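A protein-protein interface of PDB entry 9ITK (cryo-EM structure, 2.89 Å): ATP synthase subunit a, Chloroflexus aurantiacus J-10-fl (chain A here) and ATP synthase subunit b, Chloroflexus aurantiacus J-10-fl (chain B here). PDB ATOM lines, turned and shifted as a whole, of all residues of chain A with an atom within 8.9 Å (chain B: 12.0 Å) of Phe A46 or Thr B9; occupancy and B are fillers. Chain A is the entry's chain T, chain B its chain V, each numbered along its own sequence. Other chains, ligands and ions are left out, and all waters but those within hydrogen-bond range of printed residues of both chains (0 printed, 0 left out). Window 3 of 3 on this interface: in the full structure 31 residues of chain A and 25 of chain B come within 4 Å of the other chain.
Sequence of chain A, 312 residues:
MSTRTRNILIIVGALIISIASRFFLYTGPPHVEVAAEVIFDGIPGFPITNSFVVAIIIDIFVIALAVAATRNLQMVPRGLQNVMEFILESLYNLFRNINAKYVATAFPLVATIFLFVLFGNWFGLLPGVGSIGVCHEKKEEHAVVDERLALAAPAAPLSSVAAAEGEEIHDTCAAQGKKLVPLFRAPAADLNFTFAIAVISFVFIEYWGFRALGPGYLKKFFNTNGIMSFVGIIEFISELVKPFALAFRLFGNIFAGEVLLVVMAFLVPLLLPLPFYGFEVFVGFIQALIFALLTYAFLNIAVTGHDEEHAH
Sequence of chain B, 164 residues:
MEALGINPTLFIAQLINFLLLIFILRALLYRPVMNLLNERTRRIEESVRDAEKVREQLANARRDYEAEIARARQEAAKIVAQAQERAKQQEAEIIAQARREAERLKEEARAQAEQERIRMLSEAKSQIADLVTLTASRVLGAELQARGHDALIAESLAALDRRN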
ATOM      1  N   ILE A  39       7.987 -24.003  19.315  1.00  0.00           N
ATOM      2  CA  ILE A  39       8.275 -22.559  19.069  1.00  0.00           C
ATOM      3  C   ILE A  39       9.310 -22.435  17.946  1.00  0.00           C
ATOM      4  O   ILE A  39       9.022 -21.727  16.963  1.00  0.00           O
ATOM      5  CB  ILE A  39       8.730 -21.851  20.365  1.00  0.00           C
ATOM      6  CG1 ILE A  39       9.000 -20.364  20.127  1.00  0.00           C
ATOM      7  CG2 ILE A  39       9.929 -22.554  20.983  1.00  0.00           C
ATOM      8  CD1 ILE A  39       9.302 -19.584  21.385  1.00  0.00           C
ATOM      9  N   ASP A  41      11.435 -20.647  17.894  1.00  0.00           N
ATOM     10  CA  ASP A  41      11.715 -19.186  17.869  1.00  0.00           C
ATOM     11  C   ASP A  41      11.643 -18.665  16.430  1.00  0.00           C
ATOM     12  O   ASP A  41      10.680 -19.019  15.720  1.00  0.00           O
ATOM     13  CB  ASP A  41      13.065 -18.865  18.515  1.00  0.00           C
ATOM     14  CG  ASP A  41      13.172 -19.339  19.954  1.00  0.00           C
ATOM     15  OD1 ASP A  41      12.262 -20.064  20.402  1.00  0.00           O
ATOM     16  OD2 ASP A  41      14.166 -18.979  20.615  1.00  0.00           O
ATOM     17  N   GLY A  42      12.625 -17.859  16.023  1.00  0.00           N
ATOM     18  CA  GLY A  42      12.636 -17.266  14.671  1.00  0.00           C
ATOM     19  C   GLY A  42      12.745 -15.753  14.724  1.00  0.00           C
ATOM     20  O   GLY A  42      13.098 -15.153  13.690  1.00  0.00           O
ATOM     21  N   ILE A  43      12.455 -15.155  15.884  1.00  0.00           N
ATOM     22  CA  ILE A  43      12.572 -13.674  16.046  1.00  0.00           C
ATOM     23  C   ILE A  43      13.381 -13.370  17.312  1.00  0.00           C
ATOM     24  O   ILE A  43      13.048 -13.928  18.377  1.00  0.00           O
ATOM     25  CB  ILE A  43      11.183 -13.007  16.077  1.00  0.00           C
ATOM     26  CG1 ILE A  43      10.613 -12.837  14.667  1.00  0.00           C
ATOM     27  CG2 ILE A  43      11.235 -11.682  16.820  1.00  0.00           C
ATOM     28  CD1 ILE A  43      11.496 -12.029  13.746  1.00  0.00           C
ATOM     29  N   PRO A  44      14.419 -12.509  17.241  1.00  0.00           N
ATOM     30  CA  PRO A  44      15.199 -12.132  18.423  1.00  0.00           C
ATOM     31  C   PRO A  44      14.395 -11.187  19.327  1.00  0.00           C
ATOM     32  O   PRO A  44      13.380 -10.683  18.883  1.00  0.00           O
ATOM     33  CB  PRO A  44      16.404 -11.392  17.827  1.00  0.00           C
ATOM     34  CG  PRO A  44      15.869 -10.810  16.538  1.00  0.00           C
ATOM     35  CD  PRO A  44      14.895 -11.849  16.023  1.00  0.00           C
ATOM     36  N   GLY A  45      14.866 -10.971  20.559  1.00  0.00           N
ATOM     37  CA  GLY A  45      14.132 -10.112  21.509  1.00  0.00           C
ATOM     38  C   GLY A  45      12.870 -10.796  21.997  1.00  0.00           C
ATOM     39  O   GLY A  45      12.798 -11.108  23.201  1.00  0.00           O
ATOM     40  N   PHE A  46      11.909 -11.027  21.097  1.00  0.00           N
ATOM     41  CA  PHE A  46      10.689 -11.735  21.475  1.00  0.00           C
ATOM     42  C   PHE A  46      10.586 -13.024  20.673  1.00  0.00           C
ATOM     43  O   PHE A  46      10.231 -12.988  19.484  1.00  0.00           O
ATOM     44  CB  PHE A  46       9.456 -10.858  21.242  1.00  0.00           C
ATOM     45  CG  PHE A  46       8.160 -11.618  21.270  1.00  0.00           C
ATOM     46  CD1 PHE A  46       7.728 -12.232  22.435  1.00  0.00           C
ATOM     47  CD2 PHE A  46       7.376 -11.718  20.134  1.00  0.00           C
ATOM     48  CE1 PHE A  46       6.537 -12.933  22.464  1.00  0.00           C
ATOM     49  CE2 PHE A  46       6.183 -12.417  20.158  1.00  0.00           C
ATOM     50  CZ  PHE A  46       5.764 -13.026  21.325  1.00  0.00           C
ATOM     51  N   PRO A  47      10.897 -14.179  21.259  1.00  0.00           N
ATOM     52  CA  PRO A  47      10.768 -15.439  20.518  1.00  0.00           C
ATOM     53  C   PRO A  47       9.331 -15.676  20.078  1.00  0.00           C
ATOM     54  O   PRO A  47       8.379 -15.350  20.789  1.00  0.00           O
ATOM     55  CB  PRO A  47      11.233 -16.496  21.528  1.00  0.00           C
ATOM     56  CG  PRO A  47      12.064 -15.742  22.517  1.00  0.00           C
ATOM     57  CD  PRO A  47      11.445 -14.383  22.610  1.00  0.00           C
ATOM     58  N   ILE A  48       9.184 -16.251  18.888  1.00  0.00           N
ATOM     59  CA  ILE A  48       7.882 -16.488  18.278  1.00  0.00           C
ATOM     60  C   ILE A  48       7.762 -17.965  17.933  1.00  0.00           C
ATOM     61  O   ILE A  48       8.736 -18.596  17.509  1.00  0.00           O
ATOM     62  CB  ILE A  48       7.671 -15.613  17.025  1.00  0.00           C
ATOM     63  CG1 ILE A  48       8.772 -15.871  15.992  1.00  0.00           C
ATOM     64  CG2 ILE A  48       7.625 -14.142  17.404  1.00  0.00           C
ATOM     65  CD1 ILE A  48       8.470 -15.305  14.624  1.00  0.00           C
ATOM     66  N   THR A  49       6.568 -18.515  18.134  1.00  0.00           N
ATOM     67  CA  THR A  49       6.305 -19.893  17.746  1.00  0.00           C
ATOM     68  C   THR A  49       6.386 -20.039  16.234  1.00  0.00           C
ATOM     69  O   THR A  49       6.059 -19.114  15.486  1.00  0.00           O
ATOM     70  CB  THR A  49       4.928 -20.337  18.237  1.00  0.00           C
ATOM     71  OG1 THR A  49       3.953 -19.349  17.885  1.00  0.00           O
ATOM     72  CG2 THR A  49       4.937 -20.531  19.744  1.00  0.00           C
ATOM     73  N   PHE A  52       3.783 -19.064  12.961  1.00  0.00           N
ATOM     74  CA  PHE A  52       3.848 -17.971  12.001  1.00  0.00           C
ATOM     75  C   PHE A  52       4.690 -18.337  10.787  1.00  0.00           C
ATOM     76  O   PHE A  52       4.523 -17.738   9.721  1.00  0.00           O
ATOM     77  CB  PHE A  52       4.405 -16.717  12.674  1.00  0.00           C
ATOM     78  CG  PHE A  52       3.360 -15.879  13.351  1.00  0.00           C
ATOM     79  CD1 PHE A  52       2.586 -14.992  12.625  1.00  0.00           C
ATOM     80  CD2 PHE A  52       3.151 -15.980  14.716  1.00  0.00           C
ATOM     81  CE1 PHE A  52       1.624 -14.221  13.247  1.00  0.00           C
ATOM     82  CE2 PHE A  52       2.191 -15.212  15.343  1.00  0.00           C
ATOM     83  CZ  PHE A  52       1.427 -14.331  14.607  1.00  0.00           C
ATOM     84  N   ASN A 192      -2.740 -22.304  19.477  1.00  0.00           N
ATOM     85  CA  ASN A 192      -2.776 -20.845  19.489  1.00  0.00           C
ATOM     86  C   ASN A 192      -3.447 -20.300  18.234  1.00  0.00           C
ATOM     87  O   ASN A 192      -4.220 -19.337  18.304  1.00  0.00           O
ATOM     88  CB  ASN A 192      -1.362 -20.283  19.639  1.00  0.00           C
ATOM     89  CG  ASN A 192      -0.513 -20.496  18.403  1.00  0.00           C
ATOM     90  OD1 ASN A 192      -0.473 -21.592  17.848  1.00  0.00           O
ATOM     91  ND2 ASN A 192       0.163 -19.444  17.960  1.00  0.00           N
ATOM     92  N   GLY B   5       0.709 -24.732  25.685  1.00  0.00           N
ATOM     93  CA  GLY B   5       1.534 -23.774  24.972  1.00  0.00           C
ATOM     94  C   GLY B   5       0.749 -22.597  24.427  1.00  0.00           C
ATOM     95  O   GLY B   5       1.013 -22.120  23.323  1.00  0.00           O
ATOM     96  N   ILE B   6      -0.220 -22.130  25.204  1.00  0.00           N
ATOM     97  CA  ILE B   6      -1.059 -20.998  24.829  1.00  0.00           C
ATOM     98  C   ILE B   6      -0.501 -19.766  25.537  1.00  0.00           C
ATOM     99  O   ILE B   6      -0.651 -19.600  26.750  1.00  0.00           O
ATOM    100  CB  ILE B   6      -2.533 -21.249  25.166  1.00  0.00           C
ATOM    101  CG1 ILE B   6      -3.354 -19.967  25.001  1.00  0.00           C
ATOM    102  CG2 ILE B   6      -2.691 -21.864  26.557  1.00  0.00           C
ATOM    103  CD1 ILE B   6      -4.848 -20.199  24.987  1.00  0.00           C
ATOM    104  N   ASN B   7       0.164 -18.901  24.772  1.00  0.00           N
ATOM    105  CA  ASN B   7       0.740 -17.673  25.300  1.00  0.00           C
ATOM    106  C   ASN B   7      -0.089 -16.492  24.828  1.00  0.00           C
ATOM    107  O   ASN B   7      -0.195 -16.266  23.613  1.00  0.00           O
ATOM    108  CB  ASN B   7       2.193 -17.524  24.849  1.00  0.00           C
ATOM    109  CG  ASN B   7       2.908 -16.373  25.534  1.00  0.00           C
ATOM    110  OD1 ASN B   7       2.324 -15.649  26.339  1.00  0.00           O
ATOM    111  ND2 ASN B   7       4.184 -16.200  25.213  1.00  0.00           N
ATOM    112  N   PRO B   8      -0.696 -15.723  25.737  1.00  0.00           N
ATOM    113  CA  PRO B   8      -1.556 -14.610  25.300  1.00  0.00           C
ATOM    114  C   PRO B   8      -0.843 -13.582  24.442  1.00  0.00           C
ATOM    115  O   PRO B   8      -1.485 -12.944  23.599  1.00  0.00           O
ATOM    116  CB  PRO B   8      -2.035 -14.000  26.625  1.00  0.00           C
ATOM    117  CG  PRO B   8      -1.923 -15.109  27.617  1.00  0.00           C
ATOM    118  CD  PRO B   8      -0.727 -15.913  27.197  1.00  0.00           C
ATOM    119  N   THR B   9       0.465 -13.391  24.634  1.00  0.00           N
ATOM    120  CA  THR B   9       1.193 -12.417  23.827  1.00  0.00           C
ATOM    121  C   THR B   9       1.195 -12.816  22.355  1.00  0.00           C
ATOM    122  O   THR B   9       0.848 -12.012  21.483  1.00  0.00           O
ATOM    123  CB  THR B   9       2.624 -12.266  24.347  1.00  0.00           C
ATOM    124  OG1 THR B   9       2.596 -11.774  25.692  1.00  0.00           O
ATOM    125  CG2 THR B   9       3.402 -11.293  23.475  1.00  0.00           C
ATOM    126  N   LEU B  10       1.577 -14.060  22.059  1.00  0.00           N
ATOM    127  CA  LEU B  10       1.563 -14.530  20.680  1.00  0.00           C
ATOM    128  C   LEU B  10       0.168 -14.911  20.205  1.00  0.00           C
ATOM    129  O   LEU B  10      -0.062 -14.977  18.993  1.00  0.00           O
ATOM    130  CB  LEU B  10       2.527 -15.710  20.516  1.00  0.00           C
ATOM    131  CG  LEU B  10       2.314 -16.998  21.318  1.00  0.00           C
ATOM    132  CD1 LEU B  10       1.316 -17.939  20.660  1.00  0.00           C
ATOM    133  CD2 LEU B  10       3.642 -17.699  21.543  1.00  0.00           C
ATOM    134  N   PHE B  11      -0.761 -15.176  21.127  1.00  0.00           N
ATOM    135  CA  PHE B  11      -2.146 -15.408  20.731  1.00  0.00           C
ATOM    136  C   PHE B  11      -2.741 -14.167  20.082  1.00  0.00           C
ATOM    137  O   PHE B  11      -3.427 -14.257  19.057  1.00  0.00           O
ATOM    138  CB  PHE B  11      -2.973 -15.835  21.943  1.00  0.00           C
ATOM    139  CG  PHE B  11      -4.449 -15.615  21.781  1.00  0.00           C
ATOM    140  CD1 PHE B  11      -5.195 -16.417  20.938  1.00  0.00           C
ATOM    141  CD2 PHE B  11      -5.091 -14.603  22.477  1.00  0.00           C
ATOM    142  CE1 PHE B  11      -6.554 -16.215  20.793  1.00  0.00           C
ATOM    143  CE2 PHE B  11      -6.448 -14.397  22.334  1.00  0.00           C
ATOM    144  CZ  PHE B  11      -7.181 -15.204  21.490  1.00  0.00           C
ATOM    145  N   ILE B  12      -2.483 -12.994  20.665  1.00  0.00           N
ATOM    146  CA  ILE B  12      -2.920 -11.745  20.051  1.00  0.00           C
ATOM    147  C   ILE B  12      -2.168 -11.504  18.748  1.00  0.00           C
ATOM    148  O   ILE B  12      -2.705 -10.891  17.818  1.00  0.00           O
ATOM    149  CB  ILE B  12      -2.748 -10.578  21.042  1.00  0.00           C
ATOM    150  CG1 ILE B  12      -3.591 -10.821  22.294  1.00  0.00           C
ATOM    151  CG2 ILE B  12      -3.142  -9.258  20.402  1.00  0.00           C
ATOM    152  CD1 ILE B  12      -3.277  -9.881  23.435  1.00  0.00           C
ATOM    153  N   ALA B  13      -0.927 -11.986  18.653  1.00  0.00           N
ATOM    154  CA  ALA B  13      -0.171 -11.838  17.414  1.00  0.00           C
ATOM    155  C   ALA B  13      -0.867 -12.541  16.257  1.00  0.00           C
ATOM    156  O   ALA B  13      -0.964 -11.990  15.155  1.00  0.00           O
ATOM    157  CB  ALA B  13       1.248 -12.374  17.595  1.00  0.00           C
ATOM    158  N   GLN B  14      -1.361 -13.760  16.485  1.00  0.00           N
ATOM    159  CA  GLN B  14      -2.142 -14.434  15.453  1.00  0.00           C
ATOM    160  C   GLN B  14      -3.528 -13.818  15.314  1.00  0.00           C
ATOM    161  O   GLN B  14      -4.097 -13.817  14.216  1.00  0.00           O
ATOM    162  CB  GLN B  14      -2.250 -15.927  15.757  1.00  0.00           C
ATOM    163  CG  GLN B  14      -1.118 -16.760  15.176  1.00  0.00           C
ATOM    164  CD  GLN B  14      -1.318 -17.090  13.708  1.00  0.00           C
ATOM    165  OE1 GLN B  14      -1.966 -16.347  12.972  1.00  0.00           O
ATOM    166  NE2 GLN B  14      -0.754 -18.211  13.275  1.00  0.00           N
ATOM    167  N   LEU B  15      -4.086 -13.303  16.411  1.00  0.00           N
ATOM    168  CA  LEU B  15      -5.333 -12.551  16.331  1.00  0.00           C
ATOM    169  C   LEU B  15      -5.170 -11.323  15.443  1.00  0.00           C
ATOM    170  O   LEU B  15      -6.031 -11.032  14.606  1.00  0.00           O
ATOM    171  CB  LEU B  15      -5.781 -12.148  17.737  1.00  0.00           C
ATOM    172  CG  LEU B  15      -6.928 -11.154  17.958  1.00  0.00           C
ATOM    173  CD1 LEU B  15      -8.120 -11.441  17.068  1.00  0.00           C
ATOM    174  CD2 LEU B  15      -7.346 -11.139  19.421  1.00  0.00           C
ATOM    175  N   ILE B  16      -4.065 -10.594  15.611  1.00  0.00           N
ATOM    176  CA  ILE B  16      -3.810  -9.423  14.780  1.00  0.00           C
ATOM    177  C   ILE B  16      -3.478  -9.838  13.353  1.00  0.00           C
ATOM    178  O   ILE B  16      -3.944  -9.219  12.389  1.00  0.00           O
ATOM    179  CB  ILE B  16      -2.691  -8.568  15.401  1.00  0.00           C
ATOM    180  CG1 ILE B  16      -3.202  -7.863  16.659  1.00  0.00           C
ATOM    181  CG2 ILE B  16      -2.156  -7.563  14.392  1.00  0.00           C
ATOM    182  CD1 ILE B  16      -4.431  -7.010  16.426  1.00  0.00           C
ATOM    183  N   ASN B  17      -2.675 -10.893  13.192  1.00  0.00           N
ATOM    184  CA  ASN B  17      -2.231 -11.289  11.860  1.00  0.00           C
ATOM    185  C   ASN B  17      -3.405 -11.702  10.982  1.00  0.00           C
ATOM    186  O   ASN B  17      -3.551 -11.216   9.856  1.00  0.00           O
ATOM    187  CB  ASN B  17      -1.210 -12.421  11.960  1.00  0.00           C
ATOM    188  CG  ASN B  17      -0.548 -12.727  10.631  1.00  0.00           C
ATOM    189  OD1 ASN B  17      -1.184 -13.232   9.706  1.00  0.00           O
ATOM    190  ND2 ASN B  17       0.740 -12.420  10.529  1.00  0.00           N
ATOM    191  N   PHE B  18      -4.263 -12.595  11.485  1.00  0.00           N
ATOM    192  CA  PHE B  18      -5.371 -13.078  10.668  1.00  0.00           C
ATOM    193  C   PHE B  18      -6.356 -11.968  10.334  1.00  0.00           C
ATOM    194  O   PHE B  18      -6.949 -11.976   9.249  1.00  0.00           O
ATOM    195  CB  PHE B  18      -6.089 -14.232  11.363  1.00  0.00           C
ATOM    196  CG  PHE B  18      -6.985 -15.022  10.451  1.00  0.00           C
ATOM    197  CD1 PHE B  18      -6.452 -15.912   9.535  1.00  0.00           C
ATOM    198  CD2 PHE B  18      -8.360 -14.874  10.511  1.00  0.00           C
ATOM    199  CE1 PHE B  18      -7.275 -16.640   8.696  1.00  0.00           C
ATOM    200  CE2 PHE B  18      -9.187 -15.598   9.677  1.00  0.00           C
ATOM    201  CZ  PHE B  18      -8.643 -16.482   8.767  1.00  0.00           C
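OD1 of Asn B7 sits close to N of Thr B9, 3.4 Å away.
Among the printed residues, pairs that only touch across the chains: Phe A46 with Thr B9, Thr A49 with Leu B10, Phe A52 with Ala B13, Phe A52 with Gln B14, Phe A52 with Asn B17 and Asn A192 with Leu B10.
No residue of chain B comes within 4 Å of Asp A41. No residue of chain B comes within 4 Å of Gly A42. No residue of chain B comes within 4 Å of Ile A43. No residue of chain B comes within 4 Å of Pro A44. No residue of chain B comes within 4 Å of Gly A45. Of chain B, only Thr B9 (3.6 Å) comes within 4 Å of Phe A46. No residue of chain B comes within 4 Å of Pro A47. Ile A48 touches none of the printed residues of chain B. Printed residues of chain B within 4 Å of Thr A49: Leu B10 (3.6 Å). Of the printed residues of chain B, Asn A192 touches Leu B10. Gly B5 touches none of the printed residues of chain A. No residue of chain A comes within 4 Å of Pro B8. Of the printed residues of chain A, Gln B14 touches Phe A52. The nearest residue of chain B that does not touch Phe A46 is Leu B10 (4.3 Å). The nearest residue of chain A that does not touch Thr B9 is Pro A47 (7.0 Å). The nearest printed residue of chain A that does not touch Ala B13 is Phe A46 (5.6 Å).
Of the 14 printed residues of chain B, 5 touch a printed residue of chain A. Hydrophobic or aromatic side chains of chain B that line the printed part of chain A: Leu B10 and Ala B13. Along chain B the printed residues that touch a printed residue of chain A span positions 9 to 17. Hydrophobic or aromatic side chains of chain A that line the printed part of chain B: Phe A46 and Phe A52. Among the printed residues, 6 pairs touch across the chains. Among the printed residues, no Asp or Glu carboxylate lies within 4 Å of a Lys or Arg side-chain nitrogen of the other chain.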
